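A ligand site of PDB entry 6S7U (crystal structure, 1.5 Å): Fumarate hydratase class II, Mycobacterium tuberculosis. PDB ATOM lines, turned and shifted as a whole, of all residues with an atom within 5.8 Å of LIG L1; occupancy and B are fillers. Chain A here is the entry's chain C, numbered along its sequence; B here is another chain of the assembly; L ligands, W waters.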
ATOM      1  N   LEU A 303      21.258 -33.907  30.892  1.00  0.00           N
ATOM      2  CA  LEU A 303      21.772 -33.219  29.708  1.00  0.00           C
ATOM      3  C   LEU A 303      20.776 -33.294  28.577  1.00  0.00           C
ATOM      4  O   LEU A 303      20.482 -32.239  28.003  1.00  0.00           O
ATOM      5  CB  LEU A 303      23.122 -33.771  29.250  1.00  0.00           C
ATOM      6  CG  LEU A 303      23.694 -33.081  28.034  1.00  0.00           C
ATOM      7  CD1 LEU A 303      24.032 -31.632  28.351  1.00  0.00           C
ATOM      8  CD2 LEU A 303      24.906 -33.823  27.511  1.00  0.00           C
ATOM      9  N   THR A 304      20.249 -34.467  28.245  1.00  0.00           N
ATOM     10  CA  THR A 304      19.597 -34.606  26.928  1.00  0.00           C
ATOM     11  C   THR A 304      18.064 -34.536  27.032  1.00  0.00           C
ATOM     12  O   THR A 304      17.454 -34.593  25.975  1.00  0.00           O
ATOM     13  CB  THR A 304      20.041 -35.852  26.185  1.00  0.00           C
ATOM     14  OG1 THR A 304      19.440 -37.021  26.710  1.00  0.00           O
ATOM     15  CG2 THR A 304      21.549 -36.001  26.233  1.00  0.00           C
ATOM     16  N   GLY A 305      17.514 -34.377  28.228  1.00  0.00           N
ATOM     17  CA  GLY A 305      16.059 -34.289  28.428  1.00  0.00           C
ATOM     18  C   GLY A 305      15.591 -32.853  28.642  1.00  0.00           C
ATOM     19  O   GLY A 305      16.213 -31.908  28.133  1.00  0.00           O
ATOM     20  N   LEU A 306      14.506 -32.691  29.362  1.00  0.00           N
ATOM     21  CA  LEU A 306      13.917 -31.352  29.511  1.00  0.00           C
ATOM     22  C   LEU A 306      14.623 -30.574  30.637  1.00  0.00           C
ATOM     23  O   LEU A 306      14.609 -29.323  30.534  1.00  0.00           O
ATOM     24  CB  LEU A 306      12.429 -31.446  29.831  1.00  0.00           C
ATOM     25  CG  LEU A 306      11.621 -32.283  28.821  1.00  0.00           C
ATOM     26  CD1 LEU A 306      10.131 -32.192  29.128  1.00  0.00           C
ATOM     27  CD2 LEU A 306      11.901 -31.845  27.403  1.00  0.00           C
ATOM     28  N   LEU A 429      16.866 -18.911  17.526  1.00  0.00           N
ATOM     29  CA  LEU A 429      17.032 -20.380  17.627  1.00  0.00           C
ATOM     30  C   LEU A 429      18.450 -20.749  17.198  1.00  0.00           C
ATOM     31  O   LEU A 429      19.138 -21.513  17.919  1.00  0.00           O
ATOM     32  CB  LEU A 429      15.994 -21.045  16.730  1.00  0.00           C
ATOM     33  CG  LEU A 429      14.576 -21.135  17.291  1.00  0.00           C
ATOM     34  CD1 LEU A 429      13.719 -21.986  16.375  1.00  0.00           C
ATOM     35  CD2 LEU A 429      14.621 -21.744  18.690  1.00  0.00           C
ATOM     36  N   LYS A 430      18.892 -20.231  16.062  1.00  0.00           N
ATOM     37  CA  LYS A 430      20.213 -20.568  15.496  1.00  0.00           C
ATOM     38  C   LYS A 430      21.335 -20.121  16.440  1.00  0.00           C
ATOM     39  O   LYS A 430      22.279 -20.890  16.579  1.00  0.00           O
ATOM     40  CB  LYS A 430      20.339 -19.953  14.111  1.00  0.00           C
ATOM     41  CG  LYS A 430      21.695 -20.080  13.432  1.00  0.00           C
ATOM     42  CD  LYS A 430      21.782 -19.047  12.332  1.00  0.00           C
ATOM     43  CE  LYS A 430      23.100 -19.032  11.597  1.00  0.00           C
ATOM     44  NZ  LYS A 430      23.076 -20.085  10.569  1.00  0.00           N
ATOM     45  N   ARG A 432      21.076 -19.311  19.708  1.00  0.00           N
ATOM     46  CA  ARG A 432      20.762 -19.653  21.113  1.00  0.00           C
ATOM     47  C   ARG A 432      20.703 -18.398  21.952  1.00  0.00           C
ATOM     48  O   ARG A 432      21.368 -18.347  22.982  1.00  0.00           O
ATOM     49  CB  ARG A 432      21.768 -20.697  21.620  1.00  0.00           C
ATOM     50  CG  ARG A 432      21.511 -22.069  21.015  1.00  0.00           C
ATOM     51  CD  ARG A 432      22.549 -23.132  21.426  1.00  0.00           C
ATOM     52  NE  ARG A 432      22.156 -24.458  20.901  1.00  0.00           N
ATOM     53  CZ  ARG A 432      22.487 -24.960  19.713  1.00  0.00           C
ATOM     54  NH1 ARG A 432      23.235 -24.266  18.870  1.00  0.00           N
ATOM     55  NH2 ARG A 432      22.072 -26.176  19.371  1.00  0.00           N
ATOM     56  N   PRO B 302      10.772 -26.571  18.799  1.00  0.00           N
ATOM     57  CA  PRO B 302      12.179 -26.758  18.426  1.00  0.00           C
ATOM     58  C   PRO B 302      13.226 -26.338  19.454  1.00  0.00           C
ATOM     59  O   PRO B 302      14.398 -26.651  19.176  1.00  0.00           O
ATOM     60  CB  PRO B 302      12.287 -25.876  17.191  1.00  0.00           C
ATOM     61  CG  PRO B 302      11.355 -24.744  17.441  1.00  0.00           C
ATOM     62  CD  PRO B 302      10.186 -25.368  18.201  1.00  0.00           C
ATOM     63  N   LEU B 303      12.837 -25.705  20.563  1.00  0.00           N
ATOM     64  CA  LEU B 303      13.792 -25.190  21.574  1.00  0.00           C
ATOM     65  C   LEU B 303      13.745 -25.995  22.858  1.00  0.00           C
ATOM     66  O   LEU B 303      14.808 -26.357  23.359  1.00  0.00           O
ATOM     67  CB  LEU B 303      13.454 -23.738  21.899  1.00  0.00           C
ATOM     68  CG  LEU B 303      14.397 -23.111  22.931  1.00  0.00           C
ATOM     69  CD1 LEU B 303      15.849 -23.138  22.464  1.00  0.00           C
ATOM     70  CD2 LEU B 303      13.941 -21.711  23.339  1.00  0.00           C
ATOM     71  N   GLY B 305      12.285 -28.887  23.813  1.00  0.00           N
ATOM     72  CA  GLY B 305      12.112 -30.338  23.742  1.00  0.00           C
ATOM     73  C   GLY B 305      13.428 -31.061  23.458  1.00  0.00           C
ATOM     74  O   GLY B 305      14.492 -30.570  23.766  1.00  0.00           O
ATOM     75  N   LEU B 306      13.326 -32.260  22.916  1.00  0.00           N
ATOM     76  CA  LEU B 306      14.526 -33.069  22.684  1.00  0.00           C
ATOM     77  C   LEU B 306      15.214 -32.678  21.380  1.00  0.00           C
ATOM     78  O   LEU B 306      16.466 -32.845  21.324  1.00  0.00           O
ATOM     79  CB  LEU B 306      14.128 -34.542  22.629  1.00  0.00           C
ATOM     80  CG  LEU B 306      13.367 -35.089  23.832  1.00  0.00           C
ATOM     81  CD1 LEU B 306      13.218 -36.593  23.685  1.00  0.00           C
ATOM     82  CD2 LEU B 306      14.032 -34.741  25.141  1.00  0.00           C
ATOM     83  N   ALA B 307      14.481 -32.214  20.376  1.00  0.00           N
ATOM     84  CA  ALA B 307      15.006 -31.696  19.079  1.00  0.00           C
ATOM     85  C   ALA B 307      15.986 -32.685  18.444  1.00  0.00           C
ATOM     86  O   ALA B 307      17.024 -32.247  17.914  1.00  0.00           O
ATOM     87  CB  ALA B 307      15.650 -30.336  19.292  1.00  0.00           C
ATOM     88  N   ASN B 394      18.847 -34.353  13.318  1.00  0.00           N
ATOM     89  CA  ASN B 394      19.822 -33.263  13.643  1.00  0.00           C
ATOM     90  C   ASN B 394      21.157 -33.932  14.007  1.00  0.00           C
ATOM     91  O   ASN B 394      21.447 -34.138  15.199  1.00  0.00           O
ATOM     92  CB  ASN B 394      19.278 -32.401  14.773  1.00  0.00           C
ATOM     93  CG  ASN B 394      18.090 -31.558  14.357  1.00  0.00           C
ATOM     94  OD1 ASN B 394      18.055 -31.087  13.219  1.00  0.00           O
ATOM     95  ND2 ASN B 394      17.125 -31.331  15.261  1.00  0.00           N
ATOM     96  N   HIS B 397      24.036 -32.167  16.135  1.00  0.00           N
ATOM     97  CA  HIS B 397      23.492 -31.917  17.477  1.00  0.00           C
ATOM     98  C   HIS B 397      23.452 -33.213  18.310  1.00  0.00           C
ATOM     99  O   HIS B 397      23.865 -33.211  19.495  1.00  0.00           O
ATOM    100  CB  HIS B 397      22.170 -31.246  17.275  1.00  0.00           C
ATOM    101  CG  HIS B 397      21.586 -30.862  18.566  1.00  0.00           C
ATOM    102  ND1 HIS B 397      22.191 -29.902  19.353  1.00  0.00           N
ATOM    103  CD2 HIS B 397      20.556 -31.363  19.248  1.00  0.00           C
ATOM    104  CE1 HIS B 397      21.476 -29.775  20.439  1.00  0.00           C
ATOM    105  NE2 HIS B 397      20.470 -30.656  20.393  1.00  0.00           N
ATOM    106  N   ARG B 400      26.949 -34.140  19.322  1.00  0.00           N
ATOM    107  CA  ARG B 400      27.499 -33.231  20.351  1.00  0.00           C
ATOM    108  C   ARG B 400      26.915 -33.588  21.728  1.00  0.00           C
ATOM    109  O   ARG B 400      27.646 -33.523  22.710  1.00  0.00           O
ATOM    110  CB  ARG B 400      27.230 -31.771  19.988  1.00  0.00           C
ATOM    111  CG  ARG B 400      27.660 -30.812  21.092  1.00  0.00           C
ATOM    112  CD  ARG B 400      28.312 -29.582  20.511  1.00  0.00           C
ATOM    113  NE  ARG B 400      27.312 -28.579  20.151  1.00  0.00           N
ATOM    114  CZ  ARG B 400      27.607 -27.418  19.578  1.00  0.00           C
ATOM    115  NH1 ARG B 400      28.854 -27.119  19.304  1.00  0.00           N
ATOM    116  NH2 ARG B 400      26.639 -26.560  19.285  1.00  0.00           N
ATOM    117  N   LEU B 401      25.613 -33.826  21.830  1.00  0.00           N
ATOM    118  CA  LEU B 401      25.065 -34.189  23.135  1.00  0.00           C
ATOM    119  C   LEU B 401      25.682 -35.492  23.625  1.00  0.00           C
ATOM    120  O   LEU B 401      26.040 -35.524  24.793  1.00  0.00           O
ATOM    121  CB  LEU B 401      23.547 -34.313  23.072  1.00  0.00           C
ATOM    122  CG  LEU B 401      22.824 -32.990  22.861  1.00  0.00           C
ATOM    123  CD1 LEU B 401      21.319 -33.249  22.874  1.00  0.00           C
ATOM    124  CD2 LEU B 401      23.195 -31.969  23.926  1.00  0.00           C
ATOM    125  N   SER B 404      29.001 -34.972  25.144  1.00  0.00           N
ATOM    126  CA  SER B 404      28.970 -34.038  26.287  1.00  0.00           C
ATOM    127  C   SER B 404      28.330 -34.689  27.522  1.00  0.00           C
ATOM    128  O   SER B 404      28.172 -34.027  28.552  1.00  0.00           O
ATOM    129  CB  SER B 404      28.258 -32.812  25.889  1.00  0.00           C
ATOM    130  OG  SER B 404      28.857 -32.253  24.742  1.00  0.00           O
ATOM    131  N   ARG B 432      28.731 -26.593  29.861  1.00  0.00           N
ATOM    132  CA  ARG B 432      28.102 -26.969  28.559  1.00  0.00           C
ATOM    133  C   ARG B 432      29.192 -27.270  27.527  1.00  0.00           C
ATOM    134  O   ARG B 432      29.129 -26.811  26.360  1.00  0.00           O
ATOM    135  CB  ARG B 432      27.093 -25.903  28.123  1.00  0.00           C
ATOM    136  CG  ARG B 432      25.870 -25.858  29.026  1.00  0.00           C
ATOM    137  CD  ARG B 432      24.847 -24.838  28.570  1.00  0.00           C
ATOM    138  NE  ARG B 432      23.582 -24.927  29.302  1.00  0.00           N
ATOM    139  CZ  ARG B 432      23.302 -24.367  30.469  1.00  0.00           C
ATOM    140  NH1 ARG B 432      22.126 -24.592  31.018  1.00  0.00           N
ATOM    141  NH2 ARG B 432      24.215 -23.637  31.100  1.00  0.00           N
HETATM  142  O1  LIG L   1      23.015 -26.380  26.433  1.00  0.00           O
HETATM  143  C1  LIG L   1      17.905 -31.332  24.911  1.00  0.00           C
HETATM  144  C2  LIG L   1      19.991 -28.525  23.975  1.00  0.00           C
HETATM  145  C3  LIG L   1      19.442 -27.132  21.992  1.00  0.00           C
HETATM  146  N1  LIG L   1      19.055 -24.297  18.479  1.00  0.00           N
HETATM  147  C4  LIG L   1      18.252 -26.473  21.341  1.00  0.00           C
HETATM  148  C5  LIG L   1      18.606 -25.831  20.045  1.00  0.00           C
HETATM  149  N2  LIG L   1      24.248 -27.343  24.557  1.00  0.00           N
HETATM  150  C6  LIG L   1      18.675 -24.497  19.759  1.00  0.00           C
HETATM  151  C7  LIG L   1      19.244 -25.518  17.873  1.00  0.00           C
HETATM  152  C8  LIG L   1      18.960 -26.507  18.836  1.00  0.00           C
HETATM  153  C9  LIG L   1      19.038 -27.843  18.448  1.00  0.00           C
HETATM  154  C10 LIG L   1      19.382 -28.163  17.151  1.00  0.00           C
HETATM  155  C11 LIG L   1      19.654 -27.173  16.224  1.00  0.00           C
HETATM  156  C12 LIG L   1      19.588 -25.838  16.577  1.00  0.00           C
HETATM  157  S1  LIG L   1      23.389 -27.641  25.890  1.00  0.00           S
HETATM  158  O2  LIG L   1      24.151 -28.552  26.670  1.00  0.00           O
HETATM  159  C13 LIG L   1      25.042 -28.435  23.976  1.00  0.00           C
HETATM  160  C14 LIG L   1      24.820 -28.676  22.501  1.00  0.00           C
HETATM  161  C15 LIG L   1      24.615 -27.404  21.732  1.00  0.00           C
HETATM  162  C16 LIG L   1      25.619 -26.314  22.050  1.00  0.00           C
HETATM  163  C17 LIG L   1      25.267 -25.467  23.243  1.00  0.00           C
HETATM  164  C18 LIG L   1      24.053 -26.003  23.955  1.00  0.00           C
HETATM  165  C19 LIG L   1      21.922 -28.463  25.368  1.00  0.00           C
HETATM  166  C20 LIG L   1      21.169 -27.908  24.350  1.00  0.00           C
HETATM  167  C21 LIG L   1      19.583 -29.693  24.628  1.00  0.00           C
HETATM  168  O3  LIG L   1      18.421 -30.233  24.189  1.00  0.00           O
HETATM  169  C22 LIG L   1      20.348 -30.230  25.641  1.00  0.00           C
HETATM  170  C23 LIG L   1      21.526 -29.613  26.017  1.00  0.00           C
HETATM  171  N3  LIG L   1      19.139 -28.011  22.970  1.00  0.00           N
HETATM  172  O4  LIG L   1      20.586 -26.868  21.645  1.00  0.00           O
HETATM  173  O1  LG2 L   2      21.117 -24.522  23.874  1.00  0.00           O
HETATM  174  C1  LG2 L   2      15.834 -28.684  26.536  1.00  0.00           C
HETATM  175  C2  LG2 L   2      18.948 -26.852  26.929  1.00  0.00           C
HETATM  176  C3  LG2 L   2      20.494 -27.370  28.772  1.00  0.00           C
HETATM  177  N1  LG2 L   2      23.807 -27.795  31.847  1.00  0.00           N
HETATM  178  C4  LG2 L   2      21.059 -28.555  29.507  1.00  0.00           C
HETATM  179  C5  LG2 L   2      21.969 -28.180  30.643  1.00  0.00           C
HETATM  180  N2  LG2 L   2      20.611 -22.862  25.593  1.00  0.00           N
HETATM  181  C6  LG2 L   2      23.328 -28.245  30.653  1.00  0.00           C
HETATM  182  C7  LG2 L   2      22.757 -27.417  32.634  1.00  0.00           C
HETATM  183  C8  LG2 L   2      21.577 -27.658  31.917  1.00  0.00           C
HETATM  184  C9  LG2 L   2      20.355 -27.342  32.505  1.00  0.00           C
HETATM  185  C10 LG2 L   2      20.336 -26.798  33.779  1.00  0.00           C
HETATM  186  C11 LG2 L   2      21.505 -26.566  34.478  1.00  0.00           C
HETATM  187  C12 LG2 L   2      22.736 -26.882  33.913  1.00  0.00           C
HETATM  188  S1  LG2 L   2      20.006 -23.864  24.472  1.00  0.00           S
HETATM  189  O2  LG2 L   2      19.119 -23.107  23.668  1.00  0.00           O
HETATM  190  C13 LG2 L   2      21.954 -23.219  26.091  1.00  0.00           C
HETATM  191  C14 LG2 L   2      23.002 -22.187  25.740  1.00  0.00           C
HETATM  192  C15 LG2 L   2      22.811 -20.853  26.390  1.00  0.00           C
HETATM  193  C16 LG2 L   2      21.408 -20.265  26.314  1.00  0.00           C
HETATM  194  C17 LG2 L   2      20.331 -20.924  27.147  1.00  0.00           C
HETATM  195  C18 LG2 L   2      19.714 -22.159  26.531  1.00  0.00           C
HETATM  196  C19 LG2 L   2      19.058 -25.091  25.312  1.00  0.00           C
HETATM  197  C20 LG2 L   2      19.640 -25.795  26.356  1.00  0.00           C
HETATM  198  C21 LG2 L   2      17.669 -27.170  26.455  1.00  0.00           C
HETATM  199  O3  LG2 L   2      17.067 -28.230  27.075  1.00  0.00           O
HETATM  200  C22 LG2 L   2      17.092 -26.432  25.448  1.00  0.00           C
HETATM  201  C23 LG2 L   2      17.793 -25.394  24.867  1.00  0.00           C
HETATM  202  N3  LG2 L   2      19.471 -27.658  27.963  1.00  0.00           N
HETATM  203  O4  LG2 L   2      20.949 -26.250  28.919  1.00  0.00           O
HETATM  204  O   HOH W   1      15.981 -27.186  17.037  1.00  0.00           O
HETATM  205  O   HOH W   2      18.327 -30.881  21.602  1.00  0.00           O
HETATM  206  O   HOH W   3      18.193 -23.376  14.567  1.00  0.00           O
HETATM  207  O   HOH W   4      16.269 -28.647  22.671  1.00  0.00           O
HETATM  208  O   HOH W   5      26.821 -29.414  27.006  1.00  0.00           O
HETATM  209  O   HOH W   6      24.887 -28.554  18.523  1.00  0.00           O
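Leu 303 of chain A touches LIG L1.
Thr 304 touches LIG L1 (O to C1, 3.5 Å).
Gly 305 of chain A touches LIG L1 (O to C1, 3.7 Å).
Leu 303 of chain B touches LIG L1 (O to C4, 3.99 Å).
O of Gly 305 of chain B touches C1 of LIG L1 (3.7 Å).
His 397 of chain B touches LIG L1.
Arg 400 of chain B touches LIG L1.
CD2 of Leu 401 of chain B touches C23 of LIG L1 (3.6 Å).
The guanidinium group (NH2) of Arg 432 of chain A sits at hydrogen-bond distance from an oxygen (O4) of LIG L1 (2.8 Å).
N1 of LIG L1 lies within hydrogen-bond range of O of Leu 429, at 2.8 Å.
An oxygen (O1) of LIG L1 sits close to the guanidinium group (NE) of Arg 432 of chain B (3.3 Å).
NE of Arg 432 of chain A lies within hydrogen-bond range of O1 of LG2 L2, at 3.1 Å.
An oxygen (O4) of LG2 L2 is in hydrogen-bond range of the guanidinium group of Arg 432 of chain B, at 2.9 Å.
Water W2 lies within hydrogen-bond range of a ring nitrogen (NE2) of His 397 of chain B (2.5 Å), an oxygen (O3) of LIG L1 (2.7 Å) and the backbone carbonyl oxygen of Leu 306 of chain B (2.7 Å).
Water W4 lies within hydrogen-bond range of the backbone carbonyl oxygen of Leu 303 of chain B (2.8 Å), the backbone carbonyl oxygen of Gly 305 of chain B (2.8 Å) and a nitrogen (N3) of LIG L1 (3.0 Å).
Water W6 lies within hydrogen-bond range of the guanidinium group of Arg 400 of chain B (2.8 Å) and a ring nitrogen (ND1) of His 397 of chain B (3.1 Å).
O of Arg 400 of chain B sits at hydrogen-bond distance from OG of Ser 404 of chain B, at 2.7 Å.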
